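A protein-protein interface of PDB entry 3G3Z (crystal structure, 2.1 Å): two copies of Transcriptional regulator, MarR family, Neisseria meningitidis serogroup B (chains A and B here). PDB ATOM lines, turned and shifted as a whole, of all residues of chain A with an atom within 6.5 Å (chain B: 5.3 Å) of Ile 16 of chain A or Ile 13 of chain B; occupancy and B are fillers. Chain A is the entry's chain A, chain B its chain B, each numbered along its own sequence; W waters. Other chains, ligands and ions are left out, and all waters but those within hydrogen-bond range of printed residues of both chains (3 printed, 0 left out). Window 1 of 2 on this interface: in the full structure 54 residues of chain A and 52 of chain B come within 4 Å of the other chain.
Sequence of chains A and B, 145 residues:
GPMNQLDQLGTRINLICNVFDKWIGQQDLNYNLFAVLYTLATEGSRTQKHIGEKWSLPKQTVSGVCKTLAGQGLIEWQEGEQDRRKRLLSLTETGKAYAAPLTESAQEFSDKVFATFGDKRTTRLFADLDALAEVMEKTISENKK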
ATOM      1  N   THR A  11     -24.420 -15.206  18.258  1.00  0.00           N
ATOM      2  CA  THR A  11     -23.357 -14.622  17.445  1.00  0.00           C
ATOM      3  C   THR A  11     -22.991 -15.561  16.290  1.00  0.00           C
ATOM      4  O   THR A  11     -22.694 -15.106  15.192  1.00  0.00           O
ATOM      5  CB  THR A  11     -22.089 -14.307  18.258  1.00  0.00           C
ATOM      6  OG1 THR A  11     -21.584 -15.517  18.839  1.00  0.00           O
ATOM      7  CG2 THR A  11     -22.356 -13.282  19.359  1.00  0.00           C
ATOM      8  N   ARG A  12     -23.017 -16.868  16.541  1.00  0.00           N
ATOM      9  CA  ARG A  12     -22.524 -17.847  15.555  1.00  0.00           C
ATOM     10  C   ARG A  12     -23.503 -18.177  14.462  1.00  0.00           C
ATOM     11  O   ARG A  12     -23.090 -18.457  13.344  1.00  0.00           O
ATOM     12  CB  ARG A  12     -22.055 -19.141  16.232  1.00  0.00           C
ATOM     13  CG  ARG A  12     -20.651 -19.064  16.740  1.00  0.00           C
ATOM     14  CD  ARG A  12     -20.354 -20.165  17.750  1.00  0.00           C
ATOM     15  NE  ARG A  12     -19.002 -20.016  18.276  1.00  0.00           N
ATOM     16  CZ  ARG A  12     -18.656 -19.160  19.237  1.00  0.00           C
ATOM     17  NH1 ARG A  12     -19.564 -18.374  19.803  1.00  0.00           N
ATOM     18  NH2 ARG A  12     -17.397 -19.095  19.640  1.00  0.00           N
ATOM     19  N   ILE A  13     -24.794 -18.196  14.782  1.00  0.00           N
ATOM     20  CA  ILE A  13     -25.815 -18.424  13.747  1.00  0.00           C
ATOM     21  C   ILE A  13     -25.932 -17.204  12.847  1.00  0.00           C
ATOM     22  O   ILE A  13     -26.113 -17.333  11.633  1.00  0.00           O
ATOM     23  CB  ILE A  13     -27.201 -18.849  14.326  1.00  0.00           C
ATOM     24  CG1 ILE A  13     -27.792 -17.766  15.250  1.00  0.00           C
ATOM     25  CG2 ILE A  13     -27.078 -20.225  15.020  1.00  0.00           C
ATOM     26  CD1 ILE A  13     -29.243 -17.991  15.679  1.00  0.00           C
ATOM     27  N   ASN A  14     -25.803 -16.015  13.441  1.00  0.00           N
ATOM     28  CA  ASN A  14     -25.826 -14.773  12.668  1.00  0.00           C
ATOM     29  C   ASN A  14     -24.602 -14.613  11.776  1.00  0.00           C
ATOM     30  O   ASN A  14     -24.691 -13.992  10.730  1.00  0.00           O
ATOM     31  CB  ASN A  14     -26.018 -13.562  13.575  1.00  0.00           C
ATOM     32  CG  ASN A  14     -27.486 -13.260  13.829  1.00  0.00           C
ATOM     33  OD1 ASN A  14     -28.141 -12.571  13.039  1.00  0.00           O
ATOM     34  ND2 ASN A  14     -28.009 -13.757  14.945  1.00  0.00           N
ATOM     35  N   LEU A  15     -23.472 -15.204  12.174  1.00  0.00           N
ATOM     36  CA  LEU A  15     -22.273 -15.209  11.330  1.00  0.00           C
ATOM     37  C   LEU A  15     -22.473 -16.113  10.103  1.00  0.00           C
ATOM     38  O   LEU A  15     -22.203 -15.701   8.976  1.00  0.00           O
ATOM     39  CB  LEU A  15     -21.030 -15.630  12.135  1.00  0.00           C
ATOM     40  CG  LEU A  15     -19.685 -15.841  11.421  1.00  0.00           C
ATOM     41  CD1 LEU A  15     -19.211 -14.581  10.693  1.00  0.00           C
ATOM     42  CD2 LEU A  15     -18.622 -16.306  12.417  1.00  0.00           C
ATOM     43  N   ILE A  16     -22.951 -17.335  10.317  1.00  0.00           N
ATOM     44  CA  ILE A  16     -23.231 -18.234   9.193  1.00  0.00           C
ATOM     45  C   ILE A  16     -24.226 -17.563   8.236  1.00  0.00           C
ATOM     46  O   ILE A  16     -23.976 -17.472   7.024  1.00  0.00           O
ATOM     47  CB  ILE A  16     -23.746 -19.620   9.667  1.00  0.00           C
ATOM     48  CG1 ILE A  16     -22.793 -20.250  10.690  1.00  0.00           C
ATOM     49  CG2 ILE A  16     -23.936 -20.558   8.498  1.00  0.00           C
ATOM     50  CD1 ILE A  16     -21.422 -20.644  10.162  1.00  0.00           C
ATOM     51  N   CYS A  17     -25.332 -17.066   8.787  1.00  0.00           N
ATOM     52  CA  CYS A  17     -26.346 -16.344   8.007  1.00  0.00           C
ATOM     53  C   CYS A  17     -25.728 -15.203   7.184  1.00  0.00           C
ATOM     54  O   CYS A  17     -26.010 -15.060   5.998  1.00  0.00           O
ATOM     55  CB  CYS A  17     -27.431 -15.807   8.941  1.00  0.00           C
ATOM     56  SG  CYS A  17     -28.859 -15.098   8.099  1.00  0.00           S
ATOM     57  N   ASN A  18     -24.871 -14.409   7.818  1.00  0.00           N
ATOM     58  CA  ASN A  18     -24.129 -13.341   7.141  1.00  0.00           C
ATOM     59  C   ASN A  18     -23.260 -13.854   5.978  1.00  0.00           C
ATOM     60  O   ASN A  18     -23.259 -13.282   4.876  1.00  0.00           O
ATOM     61  CB  ASN A  18     -23.238 -12.640   8.170  1.00  0.00           C
ATOM     62  CG  ASN A  18     -22.679 -11.341   7.667  1.00  0.00           C
ATOM     63  OD1 ASN A  18     -23.418 -10.381   7.421  1.00  0.00           O
ATOM     64  ND2 ASN A  18     -21.362 -11.285   7.529  1.00  0.00           N
ATOM     65  N   VAL A  19     -22.516 -14.926   6.246  1.00  0.00           N
ATOM     66  CA  VAL A  19     -21.548 -15.472   5.300  1.00  0.00           C
ATOM     67  C   VAL A  19     -22.265 -16.112   4.117  1.00  0.00           C
ATOM     68  O   VAL A  19     -21.791 -16.021   2.988  1.00  0.00           O
ATOM     69  CB  VAL A  19     -20.545 -16.453   5.994  1.00  0.00           C
ATOM     70  CG1 VAL A  19     -19.640 -17.124   4.985  1.00  0.00           C
ATOM     71  CG2 VAL A  19     -19.682 -15.689   7.012  1.00  0.00           C
ATOM     72  N   PHE A  20     -23.401 -16.755   4.391  1.00  0.00           N
ATOM     73  CA  PHE A  20     -24.284 -17.254   3.356  1.00  0.00           C
ATOM     74  C   PHE A  20     -24.781 -16.115   2.462  1.00  0.00           C
ATOM     75  O   PHE A  20     -24.787 -16.245   1.233  1.00  0.00           O
ATOM     76  CB  PHE A  20     -25.469 -18.011   3.980  1.00  0.00           C
ATOM     77  CG  PHE A  20     -26.317 -18.739   2.979  1.00  0.00           C
ATOM     78  CD1 PHE A  20     -25.816 -19.839   2.292  1.00  0.00           C
ATOM     79  CD2 PHE A  20     -27.623 -18.332   2.726  1.00  0.00           C
ATOM     80  CE1 PHE A  20     -26.599 -20.508   1.367  1.00  0.00           C
ATOM     81  CE2 PHE A  20     -28.419 -19.006   1.804  1.00  0.00           C
ATOM     82  CZ  PHE A  20     -27.908 -20.087   1.121  1.00  0.00           C
ATOM     83  N   ASP A  21     -25.202 -15.008   3.080  1.00  0.00           N
ATOM     84  CA  ASP A  21     -25.619 -13.827   2.340  1.00  0.00           C
ATOM     85  C   ASP A  21     -24.485 -13.214   1.525  1.00  0.00           C
ATOM     86  O   ASP A  21     -24.711 -12.700   0.435  1.00  0.00           O
ATOM     87  CB  ASP A  21     -26.195 -12.768   3.281  1.00  0.00           C
ATOM     88  CG  ASP A  21     -27.665 -12.976   3.558  1.00  0.00           C
ATOM     89  OD1 ASP A  21     -28.220 -12.240   4.401  1.00  0.00           O
ATOM     90  OD2 ASP A  21     -28.272 -13.874   2.935  1.00  0.00           O
ATOM     91  N   LEU A 125     -24.770 -31.192  13.079  1.00  0.00           N
ATOM     92  CA  LEU A 125     -25.058 -29.766  13.127  1.00  0.00           C
ATOM     93  C   LEU A 125     -26.535 -29.500  12.855  1.00  0.00           C
ATOM     94  O   LEU A 125     -27.161 -28.711  13.557  1.00  0.00           O
ATOM     95  CB  LEU A 125     -24.170 -28.987  12.153  1.00  0.00           C
ATOM     96  CG  LEU A 125     -24.379 -27.464  12.151  1.00  0.00           C
ATOM     97  CD1 LEU A 125     -23.686 -26.798  13.342  1.00  0.00           C
ATOM     98  CD2 LEU A 125     -23.888 -26.877  10.857  1.00  0.00           C
ATOM     99  N   LEU A 129     -29.249 -27.856  15.462  1.00  0.00           N
ATOM    100  CA  LEU A 129     -29.931 -26.622  15.074  1.00  0.00           C
ATOM    101  C   LEU A 129     -31.437 -26.835  15.071  1.00  0.00           C
ATOM    102  O   LEU A 129     -32.188 -25.974  15.530  1.00  0.00           O
ATOM    103  CB  LEU A 129     -29.464 -26.131  13.698  1.00  0.00           C
ATOM    104  CG  LEU A 129     -28.028 -25.606  13.545  1.00  0.00           C
ATOM    105  CD1 LEU A 129     -27.679 -25.427  12.059  1.00  0.00           C
ATOM    106  CD2 LEU A 129     -27.814 -24.290  14.320  1.00  0.00           C
ATOM    107  N   LEU B   9     -28.565 -26.276   4.829  1.00  0.00           N
ATOM    108  CA  LEU B   9     -27.958 -25.406   5.830  1.00  0.00           C
ATOM    109  C   LEU B   9     -28.597 -24.020   5.781  1.00  0.00           C
ATOM    110  O   LEU B   9     -29.020 -23.485   6.805  1.00  0.00           O
ATOM    111  CB  LEU B   9     -26.445 -25.309   5.620  1.00  0.00           C
ATOM    112  CG  LEU B   9     -25.728 -24.121   6.285  1.00  0.00           C
ATOM    113  CD1 LEU B   9     -25.566 -24.337   7.779  1.00  0.00           C
ATOM    114  CD2 LEU B   9     -24.377 -23.837   5.641  1.00  0.00           C
ATOM    115  N   GLY B  10     -28.673 -23.454   4.584  1.00  0.00           N
ATOM    116  CA  GLY B  10     -29.181 -22.093   4.383  1.00  0.00           C
ATOM    117  C   GLY B  10     -30.572 -21.864   4.941  1.00  0.00           C
ATOM    118  O   GLY B  10     -30.802 -20.868   5.641  1.00  0.00           O
ATOM    119  N   THR B  11     -31.496 -22.780   4.627  1.00  0.00           N
ATOM    120  CA  THR B  11     -32.874 -22.692   5.109  1.00  0.00           C
ATOM    121  C   THR B  11     -32.894 -22.733   6.637  1.00  0.00           C
ATOM    122  O   THR B  11     -33.532 -21.887   7.284  1.00  0.00           O
ATOM    123  CB  THR B  11     -33.797 -23.813   4.519  1.00  0.00           C
ATOM    124  OG1 THR B  11     -33.230 -25.100   4.767  1.00  0.00           O
ATOM    125  CG2 THR B  11     -33.987 -23.650   3.027  1.00  0.00           C
ATOM    126  N   ARG B  12     -32.155 -23.699   7.194  1.00  0.00           N
ATOM    127  CA  ARG B  12     -32.000 -23.876   8.641  1.00  0.00           C
ATOM    128  C   ARG B  12     -31.484 -22.671   9.397  1.00  0.00           C
ATOM    129  O   ARG B  12     -32.121 -22.245  10.359  1.00  0.00           O
ATOM    130  CB  ARG B  12     -31.047 -25.020   8.944  1.00  0.00           C
ATOM    131  CG  ARG B  12     -31.735 -26.297   9.153  1.00  0.00           C
ATOM    132  CD  ARG B  12     -30.755 -27.370   9.619  1.00  0.00           C
ATOM    133  NE  ARG B  12     -31.497 -28.615   9.744  1.00  0.00           N
ATOM    134  CZ  ARG B  12     -31.819 -29.393   8.719  1.00  0.00           C
ATOM    135  NH1 ARG B  12     -31.424 -29.076   7.491  1.00  0.00           N
ATOM    136  NH2 ARG B  12     -32.524 -30.498   8.930  1.00  0.00           N
ATOM    137  N   ILE B  13     -30.307 -22.167   9.013  1.00  0.00           N
ATOM    138  CA  ILE B  13     -29.722 -21.016   9.715  1.00  0.00           C
ATOM    139  C   ILE B  13     -30.610 -19.776   9.621  1.00  0.00           C
ATOM    140  O   ILE B  13     -30.699 -18.995  10.576  1.00  0.00           O
ATOM    141  CB  ILE B  13     -28.277 -20.682   9.260  1.00  0.00           C
ATOM    142  CG1 ILE B  13     -28.167 -20.776   7.744  1.00  0.00           C
ATOM    143  CG2 ILE B  13     -27.277 -21.626   9.962  1.00  0.00           C
ATOM    144  CD1 ILE B  13     -27.380 -19.683   7.095  1.00  0.00           C
ATOM    145  N   ASN B  14     -31.269 -19.600   8.478  1.00  0.00           N
ATOM    146  CA  ASN B  14     -32.208 -18.491   8.312  1.00  0.00           C
ATOM    147  C   ASN B  14     -33.444 -18.614   9.203  1.00  0.00           C
ATOM    148  O   ASN B  14     -33.901 -17.624   9.782  1.00  0.00           O
ATOM    149  CB  ASN B  14     -32.582 -18.300   6.844  1.00  0.00           C
ATOM    150  CG  ASN B  14     -31.637 -17.357   6.142  1.00  0.00           C
ATOM    151  OD1 ASN B  14     -31.801 -16.134   6.235  1.00  0.00           O
ATOM    152  ND2 ASN B  14     -30.626 -17.910   5.440  1.00  0.00           N
ATOM    153  N   LEU B  15     -33.953 -19.838   9.319  1.00  0.00           N
ATOM    154  CA  LEU B  15     -35.009 -20.155  10.267  1.00  0.00           C
ATOM    155  C   LEU B  15     -34.572 -19.812  11.692  1.00  0.00           C
ATOM    156  O   LEU B  15     -35.256 -19.056  12.378  1.00  0.00           O
ATOM    157  CB  LEU B  15     -35.412 -21.629  10.163  1.00  0.00           C
ATOM    158  CG  LEU B  15     -36.622 -22.058  10.999  1.00  0.00           C
ATOM    159  CD1 LEU B  15     -37.894 -21.468  10.432  1.00  0.00           C
ATOM    160  CD2 LEU B  15     -36.735 -23.566  11.037  1.00  0.00           C
ATOM    161  N   ILE B  16     -33.423 -20.340  12.115  1.00  0.00           N
ATOM    162  CA  ILE B  16     -32.947 -20.153  13.488  1.00  0.00           C
ATOM    163  C   ILE B  16     -32.589 -18.688  13.832  1.00  0.00           C
ATOM    164  O   ILE B  16     -32.868 -18.239  14.946  1.00  0.00           O
ATOM    165  CB  ILE B  16     -31.822 -21.185  13.896  1.00  0.00           C
ATOM    166  CG1 ILE B  16     -31.681 -21.290  15.418  1.00  0.00           C
ATOM    167  CG2 ILE B  16     -30.485 -20.815  13.314  1.00  0.00           C
ATOM    168  CD1 ILE B  16     -31.123 -22.639  15.919  1.00  0.00           C
ATOM    169  N   CYS B  17     -31.994 -17.949  12.890  1.00  0.00           N
ATOM    170  CA  CYS B  17     -31.764 -16.499  13.084  1.00  0.00           C
ATOM    171  C   CYS B  17     -33.075 -15.711  13.281  1.00  0.00           C
ATOM    172  O   CYS B  17     -33.156 -14.803  14.125  1.00  0.00           O
ATOM    173  CB  CYS B  17     -30.945 -15.897  11.927  1.00  0.00           C
ATOM    174  SG  CYS B  17     -29.227 -16.530  11.870  1.00  0.00           S
ATOM    175  N   ASN B  18     -34.093 -16.071  12.507  1.00  0.00           N
ATOM    176  CA  ASN B  18     -35.425 -15.469  12.633  1.00  0.00           C
ATOM    177  C   ASN B  18     -36.062 -15.758  13.973  1.00  0.00           C
ATOM    178  O   ASN B  18     -36.714 -14.897  14.562  1.00  0.00           O
ATOM    179  CB  ASN B  18     -36.347 -16.000  11.540  1.00  0.00           C
ATOM    180  CG  ASN B  18     -36.311 -15.168  10.292  1.00  0.00           C
ATOM    181  OD1 ASN B  18     -35.320 -14.492  10.002  1.00  0.00           O
ATOM    182  ND2 ASN B  18     -37.401 -15.211   9.529  1.00  0.00           N
ATOM    183  N   LEU B 129     -19.781 -24.648  14.343  1.00  0.00           N
ATOM    184  CA  LEU B 129     -20.237 -23.431  13.688  1.00  0.00           C
ATOM    185  C   LEU B 129     -19.056 -22.556  13.262  1.00  0.00           C
ATOM    186  O   LEU B 129     -19.016 -22.078  12.130  1.00  0.00           O
ATOM    187  CB  LEU B 129     -21.206 -22.672  14.597  1.00  0.00           C
ATOM    188  CG  LEU B 129     -22.589 -23.318  14.687  1.00  0.00           C
ATOM    189  CD1 LEU B 129     -23.333 -22.906  15.942  1.00  0.00           C
ATOM    190  CD2 LEU B 129     -23.417 -23.011  13.429  1.00  0.00           C
ATOM    191  N   LEU B 132     -17.366 -24.231  10.399  1.00  0.00           N
ATOM    192  CA  LEU B 132     -18.236 -24.012   9.245  1.00  0.00           C
ATOM    193  C   LEU B 132     -18.021 -22.624   8.651  1.00  0.00           C
ATOM    194  O   LEU B 132     -17.803 -22.478   7.437  1.00  0.00           O
ATOM    195  CB  LEU B 132     -19.704 -24.175   9.635  1.00  0.00           C
ATOM    196  CG  LEU B 132     -20.665 -24.852   8.657  1.00  0.00           C
ATOM    197  CD1 LEU B 132     -22.049 -24.276   8.863  1.00  0.00           C
ATOM    198  CD2 LEU B 132     -20.265 -24.704   7.201  1.00  0.00           C
ATOM    199  N   ALA B 133     -18.080 -21.606   9.509  1.00  0.00           N
ATOM    200  CA  ALA B 133     -17.841 -20.233   9.079  1.00  0.00           C
ATOM    201  C   ALA B 133     -16.486 -20.097   8.373  1.00  0.00           C
ATOM    202  O   ALA B 133     -16.428 -19.534   7.282  1.00  0.00           O
ATOM    203  CB  ALA B 133     -17.968 -19.256  10.253  1.00  0.00           C
ATOM    204  N   MET B 136     -16.354 -21.583   4.775  1.00  0.00           N
ATOM    205  CA  MET B 136     -17.171 -20.747   3.916  1.00  0.00           C
ATOM    206  C   MET B 136     -16.459 -19.445   3.557  1.00  0.00           C
ATOM    207  O   MET B 136     -16.434 -19.064   2.386  1.00  0.00           O
ATOM    208  CB  MET B 136     -18.533 -20.467   4.568  1.00  0.00           C
ATOM    209  CG  MET B 136     -19.464 -21.681   4.666  1.00  0.00           C
ATOM    210  SD  MET B 136     -21.101 -21.341   5.721  1.00  0.00           S
ATOM    211  CE  MET B 136     -20.408 -19.991   6.918  1.00  0.00           C
HETATM  212  O   HOH W   1     -30.651 -13.827   4.974  1.00  0.00           O
HETATM  213  O   HOH W   2     -28.405 -15.770   5.002  1.00  0.00           O
HETATM  214  O   HOH W   3     -31.019 -13.415  15.132  1.00  0.00           O
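The side-chain sulfur of Cys 17 of chain B sits at hydrogen-bond distance from the backbone carbonyl oxygen of Ile 13 of chain A (3.2 Å).
SG of Cys 17 of chain A lies within hydrogen-bond range of OD1 of Asn 14 of chain B (3.6 Å).
ND2 of Asn 14 of chain B lies within hydrogen-bond range of O of Gly 10 of chain B (3.0 Å).
The side-chain sulfur (SG) of Cys 17 of chain B lies within hydrogen-bond range of the backbone carbonyl oxygen (O) of Ile 13 of chain B (3.1 Å).
The backbone carbonyl oxygen (O) of Asn 14 of chain B lies close to the side-chain amide oxygen (OD1) of Asn 18 of chain B.
Leu 129 of chain B touches Arg 12 of chain A (CB to CB, 3.98 Å).
Ile 13 of chain A touches Ile 16 of chain B (CD1 to O, 3.7 Å).
N of Asn 14 of chain A touches SG of Cys 17 of chain B (3.8 Å).
CG2 of Ile 13 of chain B touches CG2 of Ile 16 of chain A, 3.8 Å away.
CD1 of Ile 16 of chain A touches O of Leu 129 of chain B, 3.4 Å away.
Leu 132 of chain B touches Ile 16 of chain A (CD1 to CD1, 3.9 Å).
Ile 16 of chain A touches Ala 133 of chain B.
Cys 17 of chain A touches Cys 17 of chain B.
Met 136 of chain B touches Val 19 of chain A.
CD1 of Leu 132 of chain B touches CD2 of Leu 125 of chain A (3.8 Å).
Of chain B, only Ile 13 (3.8 Å), Leu 129 (3.4 Å), Leu 132 (3.9 Å), Ala 133 (3.5 Å) and Met 136 (3.5 Å) come within 4 Å of Ile 16 of chain A.
Asn 18 of chain A touches none of the printed residues of chain B.
Of the printed residues of chain B, Leu 125 of chain A touches Leu 129 (3.8 Å) and Leu 132 (3.8 Å).
Arg 12 of chain B touches none of the printed residues of chain A.
Of the printed residues of chain A, Ile 13 of chain B touches Ile 16 and Cys 17.
Of the printed residues of chain A, Asn 14 of chain B touches Cys 17.
Of the printed residues of chain A, Leu 129 of chain B touches Arg 12, Ile 16 and Leu 125.
Of the printed residues of chain A, Ala 133 of chain B touches Leu 15 (3.7 Å) and Ile 16 (3.5 Å).
Of the printed residues of chain A, Met 136 of chain B touches Ile 16 and Val 19.
The nearest residue of chain B that does not touch Ile 16 of chain A is Leu 9 of chain B (4.2 Å).
The nearest printed residue of chain B that does not touch Ile 13 of chain A is Ile 13 of chain B (4.6 Å).
Of the 13 printed residues of chain A, 9 touch a printed residue of chain B.
Among the printed residues, 17 pairs touch across the chains.
Among the printed residues, no Asp or Glu carboxylate lies within 4 Å of a Lys or Arg side-chain nitrogen of the other chain.
Arg 12 of chain A touches Leu 129 of chain B, but with the chains exchanged Leu 129 of chain A does not touch Arg 12 of chain B (4.4 Å).
Asn 14 of chain A touches Cys 17 of chain B, and with the chains exchanged Cys 17 of chain A touches Asn 14 of chain B.
Ile 16 of chain A touches Leu 129 of chain B, and with the chains exchanged Leu 129 of chain A touches Ile 16 of chain B.
Cys 17 of chain B touches its own counterpart, Cys 17 of chain A.
9 positions are printed for both chains.
Water W2 lies within hydrogen-bond range of the backbone carbonyl oxygen (O) of Cys 17 of chain A (2.7 Å), the side-chain carboxylate (OD2) of Asp 21 of chain A (2.8 Å) and the side-chain amide nitrogen (ND2) of Asn 14 of chain B (3.1 Å).
Water W3 bridges the backbone carbonyl oxygen of Cys 17 of chain B (2.7 Å) and the side-chain amide nitrogen of Asn 14 of chain A (3.0 Å).
Water W1 bridges the side-chain amide oxygen (OD1) of Asn 14 of chain B (2.9 Å) and the side-chain carboxylate (OD1) of Asp 21 of chain A (3.0 Å).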
